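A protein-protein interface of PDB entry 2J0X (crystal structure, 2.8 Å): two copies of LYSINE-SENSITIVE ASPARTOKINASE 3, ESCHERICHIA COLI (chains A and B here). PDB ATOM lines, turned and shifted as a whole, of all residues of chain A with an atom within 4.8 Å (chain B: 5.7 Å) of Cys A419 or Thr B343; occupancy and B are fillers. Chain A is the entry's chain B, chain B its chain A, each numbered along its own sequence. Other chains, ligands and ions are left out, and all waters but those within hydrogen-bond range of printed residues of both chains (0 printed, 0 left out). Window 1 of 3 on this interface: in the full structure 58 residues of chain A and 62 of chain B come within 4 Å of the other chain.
CA of Leu A341 touches OG1 of Thr B344, at 3.1 Å. Ile A342 touches Thr B343 (O to CA, 3.5 Å). Thr A343 touches Cys B419 (OG1 to CA, 3.7 Å). Ile A418 touches Ile B418 (O to O, 3.7 Å). Thr B343 touches Cys A419. Thr B344 touches Cys A419 (O to CB, 3.4 Å). Tyr A420 touches Met B417. CG2 of Thr B343 touches N of Ala A422, 3.7 Å away. Ala A422 touches Thr B344 (CB to C, 3.9 Å). Ala B350 touches Ala A422.
Ile A342 touches its own counterpart, Ile B342. Ile A342 touches Thr B343, and with the chains exchanged Thr A343 touches Ile B342. Thr A343 touches Cys B419, and with the chains exchanged Cys A419 touches Thr B343. Ile B418 touches its own counterpart, Ile A418. Positions printed for both chains: 341, 342, 343, 417, 418 and 419.
Printed residues of chain B within 4 Å of Ile A342: Ile B342, Thr B343 and Thr B344. Of chain A, only Ile A342 (3.5 Å), Cys A419 (3.8 Å), Tyr A420 (3.2 Å) and Ala A422 (3.7 Å) come within 4 Å of Thr B343. Of the printed residues of chain A, Ser B348 touches Ala A422. The nearest printed residue of chain A that does not touch Ala B350 is Gly A421 (4.5 Å).
The backbone carbonyl oxygen (O) of Ile B342 sits at hydrogen-bond distance from the side-chain sulfur (SG) of Cys B419 (3.7 Å). N of Thr B343 sits at hydrogen-bond distance from O of Ala B350 (2.8 Å). The side-chain hydroxyl of Ser B345 lies within hydrogen-bond range of the backbone NH of Ser B348, 3.3 Å away. SG of Cys A419 sits at hydrogen-bond distance from O of Ile A342 (3.7 Å). The backbone NH of Cys A419 is in hydrogen-bond range of the backbone carbonyl oxygen of Cys A428, 2.9 Å away.
The backbone NH of Tyr A420 lies within hydrogen-bond range of the side-chain hydroxyl of Thr B343 (3.2 Å). The backbone NH (N) of Ile A342 lies within hydrogen-bond range of the side-chain hydroxyl (OG1) of Thr B344 (2.8 Å). The backbone NH (N) of Ile B418 sits at hydrogen-bond distance from the backbone carbonyl oxygen (O) of Tyr A420 (3.1 Å). The backbone carbonyl oxygen of Ile B342 lies close to the backbone carbonyl oxygen of Ile A342 (3.2 Å).
Of the 12 printed residues of chain A, 7 touch a printed residue of chain B. Hydrophobic or aromatic side chains of chain A that line the printed part of chain B: Leu A341, Ile A342 and Ala A422. Among the printed residues, 17 pairs touch across the chains. Among the printed residues, no Asp or Glu carboxylate lies within 4 Å of a Lys or Arg side-chain nitrogen of the other chain.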
ATOM      1  N   LEU A 341     -26.219   0.067   8.173  1.00  0.00           N
ATOM      2  CA  LEU A 341     -25.651   0.153   9.514  1.00  0.00           C
ATOM      3  C   LEU A 341     -26.711   0.267  10.614  1.00  0.00           C
ATOM      4  O   LEU A 341     -27.769   0.870  10.422  1.00  0.00           O
ATOM      5  CB  LEU A 341     -24.684   1.341   9.603  1.00  0.00           C
ATOM      6  CG  LEU A 341     -23.554   1.451   8.569  1.00  0.00           C
ATOM      7  CD1 LEU A 341     -22.634   2.586   8.972  1.00  0.00           C
ATOM      8  CD2 LEU A 341     -22.767   0.147   8.492  1.00  0.00           C
ATOM      9  N   ILE A 342     -26.416  -0.329  11.766  1.00  0.00           N
ATOM     10  CA  ILE A 342     -27.316  -0.287  12.915  1.00  0.00           C
ATOM     11  C   ILE A 342     -26.528  -0.170  14.206  1.00  0.00           C
ATOM     12  O   ILE A 342     -25.588  -0.928  14.424  1.00  0.00           O
ATOM     13  CB  ILE A 342     -28.145  -1.564  13.070  1.00  0.00           C
ATOM     14  CG1 ILE A 342     -28.847  -1.910  11.765  1.00  0.00           C
ATOM     15  CG2 ILE A 342     -29.172  -1.366  14.182  1.00  0.00           C
ATOM     16  CD1 ILE A 342     -29.688  -3.165  11.871  1.00  0.00           C
ATOM     17  N   THR A 343     -26.909   0.776  15.057  1.00  0.00           N
ATOM     18  CA  THR A 343     -26.253   0.936  16.345  1.00  0.00           C
ATOM     19  C   THR A 343     -27.368   1.162  17.357  1.00  0.00           C
ATOM     20  O   THR A 343     -28.441   1.660  17.006  1.00  0.00           O
ATOM     21  CB  THR A 343     -25.230   2.097  16.345  1.00  0.00           C
ATOM     22  OG1 THR A 343     -24.426   2.007  17.529  1.00  0.00           O
ATOM     23  CG2 THR A 343     -25.932   3.455  16.281  1.00  0.00           C
ATOM     24  N   MET A 417     -20.954   8.316  14.534  1.00  0.00           N
ATOM     25  CA  MET A 417     -21.483   6.969  14.752  1.00  0.00           C
ATOM     26  C   MET A 417     -20.385   5.960  14.481  1.00  0.00           C
ATOM     27  O   MET A 417     -19.588   6.130  13.551  1.00  0.00           O
ATOM     28  CB  MET A 417     -22.699   6.699  13.838  1.00  0.00           C
ATOM     29  CG  MET A 417     -23.473   5.401  14.147  1.00  0.00           C
ATOM     30  SD  MET A 417     -25.019   5.147  13.174  1.00  0.00           S
ATOM     31  CE  MET A 417     -24.954   3.386  12.895  1.00  0.00           C
ATOM     32  N   ILE A 418     -20.333   4.920  15.306  1.00  0.00           N
ATOM     33  CA  ILE A 418     -19.319   3.889  15.138  1.00  0.00           C
ATOM     34  C   ILE A 418     -19.929   2.524  15.212  1.00  0.00           C
ATOM     35  O   ILE A 418     -20.767   2.264  16.071  1.00  0.00           O
ATOM     36  CB  ILE A 418     -18.251   3.923  16.227  1.00  0.00           C
ATOM     37  CG1 ILE A 418     -17.627   5.315  16.324  1.00  0.00           C
ATOM     38  CG2 ILE A 418     -17.194   2.881  15.908  1.00  0.00           C
ATOM     39  CD1 ILE A 418     -16.746   5.499  17.526  1.00  0.00           C
ATOM     40  N   CYS A 419     -19.506   1.659  14.300  1.00  0.00           N
ATOM     41  CA  CYS A 419     -19.973   0.284  14.274  1.00  0.00           C
ATOM     42  C   CYS A 419     -18.716  -0.559  14.302  1.00  0.00           C
ATOM     43  O   CYS A 419     -17.891  -0.492  13.391  1.00  0.00           O
ATOM     44  CB  CYS A 419     -20.787  -0.002  13.010  1.00  0.00           C
ATOM     45  SG  CYS A 419     -22.507   0.559  13.081  1.00  0.00           S
ATOM     46  N   TYR A 420     -18.566  -1.338  15.361  1.00  0.00           N
ATOM     47  CA  TYR A 420     -17.393  -2.173  15.515  1.00  0.00           C
ATOM     48  C   TYR A 420     -17.668  -3.419  16.358  1.00  0.00           C
ATOM     49  O   TYR A 420     -18.381  -3.360  17.357  1.00  0.00           O
ATOM     50  CB  TYR A 420     -16.282  -1.336  16.143  1.00  0.00           C
ATOM     51  CG  TYR A 420     -15.078  -2.139  16.524  1.00  0.00           C
ATOM     52  CD1 TYR A 420     -14.168  -2.565  15.559  1.00  0.00           C
ATOM     53  CD2 TYR A 420     -14.883  -2.533  17.848  1.00  0.00           C
ATOM     54  CE1 TYR A 420     -13.095  -3.370  15.904  1.00  0.00           C
ATOM     55  CE2 TYR A 420     -13.819  -3.335  18.204  1.00  0.00           C
ATOM     56  CZ  TYR A 420     -12.928  -3.757  17.230  1.00  0.00           C
ATOM     57  OH  TYR A 420     -11.892  -4.586  17.590  1.00  0.00           O
ATOM     58  N   GLY A 421     -17.099  -4.547  15.950  1.00  0.00           N
ATOM     59  CA  GLY A 421     -17.303  -5.779  16.694  1.00  0.00           C
ATOM     60  C   GLY A 421     -17.960  -6.877  15.879  1.00  0.00           C
ATOM     61  O   GLY A 421     -17.753  -8.064  16.122  1.00  0.00           O
ATOM     62  N   ALA A 422     -18.764  -6.488  14.903  1.00  0.00           N
ATOM     63  CA  ALA A 422     -19.432  -7.470  14.074  1.00  0.00           C
ATOM     64  C   ALA A 422     -18.403  -8.256  13.272  1.00  0.00           C
ATOM     65  O   ALA A 422     -18.471  -9.479  13.200  1.00  0.00           O
ATOM     66  CB  ALA A 422     -20.416  -6.784  13.139  1.00  0.00           C
ATOM     67  N   LEU A 427     -14.269  -1.993  10.086  1.00  0.00           N
ATOM     68  CA  LEU A 427     -14.437  -1.003  11.137  1.00  0.00           C
ATOM     69  C   LEU A 427     -14.961   0.214  10.399  1.00  0.00           C
ATOM     70  O   LEU A 427     -14.236   0.811   9.607  1.00  0.00           O
ATOM     71  CB  LEU A 427     -13.104  -0.629  11.803  1.00  0.00           C
ATOM     72  CG  LEU A 427     -13.161   0.250  13.079  1.00  0.00           C
ATOM     73  CD1 LEU A 427     -11.776   0.801  13.372  1.00  0.00           C
ATOM     74  CD2 LEU A 427     -14.120   1.419  12.917  1.00  0.00           C
ATOM     75  N   CYS A 428     -16.216   0.581  10.626  1.00  0.00           N
ATOM     76  CA  CYS A 428     -16.737   1.760   9.952  1.00  0.00           C
ATOM     77  C   CYS A 428     -17.440   2.709  10.903  1.00  0.00           C
ATOM     78  O   CYS A 428     -17.857   2.332  12.001  1.00  0.00           O
ATOM     79  CB  CYS A 428     -17.656   1.391   8.770  1.00  0.00           C
ATOM     80  SG  CYS A 428     -19.089   0.308   9.069  1.00  0.00           S
ATOM     81  N   PHE A 429     -17.538   3.958  10.473  1.00  0.00           N
ATOM     82  CA  PHE A 429     -18.160   5.000  11.268  1.00  0.00           C
ATOM     83  C   PHE A 429     -18.730   6.050  10.340  1.00  0.00           C
ATOM     84  O   PHE A 429     -18.544   6.002   9.119  1.00  0.00           O
ATOM     85  CB  PHE A 429     -17.126   5.641  12.189  1.00  0.00           C
ATOM     86  CG  PHE A 429     -15.937   6.199  11.463  1.00  0.00           C
ATOM     87  CD1 PHE A 429     -15.948   7.501  10.978  1.00  0.00           C
ATOM     88  CD2 PHE A 429     -14.815   5.407  11.234  1.00  0.00           C
ATOM     89  CE1 PHE A 429     -14.858   8.010  10.272  1.00  0.00           C
ATOM     90  CE2 PHE A 429     -13.723   5.902  10.530  1.00  0.00           C
ATOM     91  CZ  PHE A 429     -13.745   7.209  10.048  1.00  0.00           C
ATOM     92  N   LEU B 341     -27.920  -4.958  22.621  1.00  0.00           N
ATOM     93  CA  LEU B 341     -27.024  -4.255  21.714  1.00  0.00           C
ATOM     94  C   LEU B 341     -27.010  -4.847  20.305  1.00  0.00           C
ATOM     95  O   LEU B 341     -27.251  -6.039  20.106  1.00  0.00           O
ATOM     96  CB  LEU B 341     -25.606  -4.278  22.262  1.00  0.00           C
ATOM     97  CG  LEU B 341     -25.382  -3.775  23.681  1.00  0.00           C
ATOM     98  CD1 LEU B 341     -23.893  -3.755  23.962  1.00  0.00           C
ATOM     99  CD2 LEU B 341     -25.979  -2.392  23.838  1.00  0.00           C
ATOM    100  N   ILE B 342     -26.725  -3.993  19.328  1.00  0.00           N
ATOM    101  CA  ILE B 342     -26.652  -4.407  17.934  1.00  0.00           C
ATOM    102  C   ILE B 342     -25.612  -3.560  17.220  1.00  0.00           C
ATOM    103  O   ILE B 342     -25.608  -2.338  17.340  1.00  0.00           O
ATOM    104  CB  ILE B 342     -27.988  -4.210  17.203  1.00  0.00           C
ATOM    105  CG1 ILE B 342     -29.099  -4.954  17.933  1.00  0.00           C
ATOM    106  CG2 ILE B 342     -27.869  -4.695  15.756  1.00  0.00           C
ATOM    107  CD1 ILE B 342     -30.457  -4.652  17.368  1.00  0.00           C
ATOM    108  N   THR B 343     -24.722  -4.226  16.495  1.00  0.00           N
ATOM    109  CA  THR B 343     -23.680  -3.562  15.718  1.00  0.00           C
ATOM    110  C   THR B 343     -23.659  -4.269  14.373  1.00  0.00           C
ATOM    111  O   THR B 343     -23.929  -5.468  14.293  1.00  0.00           O
ATOM    112  CB  THR B 343     -22.293  -3.714  16.353  1.00  0.00           C
ATOM    113  OG1 THR B 343     -21.330  -3.006  15.567  1.00  0.00           O
ATOM    114  CG2 THR B 343     -21.892  -5.172  16.404  1.00  0.00           C
ATOM    115  N   THR B 344     -23.324  -3.544  13.316  1.00  0.00           N
ATOM    116  CA  THR B 344     -23.317  -4.155  12.001  1.00  0.00           C
ATOM    117  C   THR B 344     -22.078  -3.868  11.175  1.00  0.00           C
ATOM    118  O   THR B 344     -21.369  -2.888  11.395  1.00  0.00           O
ATOM    119  CB  THR B 344     -24.542  -3.693  11.182  1.00  0.00           C
ATOM    120  OG1 THR B 344     -24.506  -2.263  11.034  1.00  0.00           O
ATOM    121  CG2 THR B 344     -25.840  -4.116  11.872  1.00  0.00           C
ATOM    122  N   SER B 345     -21.831  -4.759  10.222  1.00  0.00           N
ATOM    123  CA  SER B 345     -20.730  -4.627   9.288  1.00  0.00           C
ATOM    124  C   SER B 345     -21.459  -4.782   7.964  1.00  0.00           C
ATOM    125  O   SER B 345     -22.683  -4.837   7.942  1.00  0.00           O
ATOM    126  CB  SER B 345     -19.695  -5.747   9.471  1.00  0.00           C
ATOM    127  OG  SER B 345     -19.850  -6.771   8.512  1.00  0.00           O
ATOM    128  N   SER B 348     -22.430  -8.789   8.005  1.00  0.00           N
ATOM    129  CA  SER B 348     -22.528  -9.455   9.292  1.00  0.00           C
ATOM    130  C   SER B 348     -23.127  -8.533  10.340  1.00  0.00           C
ATOM    131  O   SER B 348     -22.914  -7.323  10.304  1.00  0.00           O
ATOM    132  CB  SER B 348     -21.129  -9.899   9.726  1.00  0.00           C
ATOM    133  OG  SER B 348     -21.157 -10.592  10.953  1.00  0.00           O
ATOM    134  N   VAL B 349     -23.882  -9.114  11.267  1.00  0.00           N
ATOM    135  CA  VAL B 349     -24.505  -8.365  12.350  1.00  0.00           C
ATOM    136  C   VAL B 349     -24.262  -9.082  13.679  1.00  0.00           C
ATOM    137  O   VAL B 349     -24.402 -10.301  13.771  1.00  0.00           O
ATOM    138  CB  VAL B 349     -26.023  -8.234  12.161  1.00  0.00           C
ATOM    139  CG1 VAL B 349     -26.650  -9.611  12.067  1.00  0.00           C
ATOM    140  CG2 VAL B 349     -26.620  -7.488  13.339  1.00  0.00           C
ATOM    141  N   ALA B 350     -23.891  -8.317  14.703  1.00  0.00           N
ATOM    142  CA  ALA B 350     -23.633  -8.873  16.033  1.00  0.00           C
ATOM    143  C   ALA B 350     -24.544  -8.224  17.062  1.00  0.00           C
ATOM    144  O   ALA B 350     -24.667  -6.996  17.120  1.00  0.00           O
ATOM    145  CB  ALA B 350     -22.176  -8.657  16.439  1.00  0.00           C
ATOM    146  N   LEU B 351     -25.180  -9.050  17.878  1.00  0.00           N
ATOM    147  CA  LEU B 351     -26.076  -8.527  18.892  1.00  0.00           C
ATOM    148  C   LEU B 351     -25.882  -9.283  20.198  1.00  0.00           C
ATOM    149  O   LEU B 351     -25.333 -10.380  20.205  1.00  0.00           O
ATOM    150  CB  LEU B 351     -27.531  -8.656  18.433  1.00  0.00           C
ATOM    151  CG  LEU B 351     -28.127 -10.065  18.368  1.00  0.00           C
ATOM    152  CD1 LEU B 351     -29.582  -9.997  17.912  1.00  0.00           C
ATOM    153  CD2 LEU B 351     -27.325 -10.905  17.412  1.00  0.00           C
ATOM    154  N   MET B 417     -16.355  -4.541  21.152  1.00  0.00           N
ATOM    155  CA  MET B 417     -17.567  -4.034  20.505  1.00  0.00           C
ATOM    156  C   MET B 417     -17.904  -2.638  20.984  1.00  0.00           C
ATOM    157  O   MET B 417     -17.783  -2.334  22.159  1.00  0.00           O
ATOM    158  CB  MET B 417     -18.759  -4.943  20.798  1.00  0.00           C
ATOM    159  CG  MET B 417     -19.971  -4.602  19.976  1.00  0.00           C
ATOM    160  SD  MET B 417     -21.237  -5.863  20.085  1.00  0.00           S
ATOM    161  CE  MET B 417     -22.609  -4.870  20.659  1.00  0.00           C
ATOM    162  N   ILE B 418     -18.339  -1.787  20.071  1.00  0.00           N
ATOM    163  CA  ILE B 418     -18.685  -0.425  20.433  1.00  0.00           C
ATOM    164  C   ILE B 418     -20.022  -0.042  19.848  1.00  0.00           C
ATOM    165  O   ILE B 418     -20.311  -0.333  18.686  1.00  0.00           O
ATOM    166  CB  ILE B 418     -17.662   0.583  19.889  1.00  0.00           C
ATOM    167  CG1 ILE B 418     -16.292   0.320  20.501  1.00  0.00           C
ATOM    168  CG2 ILE B 418     -18.135   2.003  20.166  1.00  0.00           C
ATOM    169  CD1 ILE B 418     -15.227   1.253  19.992  1.00  0.00           C
ATOM    170  N   CYS B 419     -20.835   0.616  20.663  1.00  0.00           N
ATOM    171  CA  CYS B 419     -22.138   1.100  20.235  1.00  0.00           C
ATOM    172  C   CYS B 419     -22.147   2.592  20.544  1.00  0.00           C
ATOM    173  O   CYS B 419     -22.148   3.000  21.703  1.00  0.00           O
ATOM    174  CB  CYS B 419     -23.260   0.395  20.995  1.00  0.00           C
ATOM    175  SG  CYS B 419     -23.720  -1.212  20.331  1.00  0.00           S
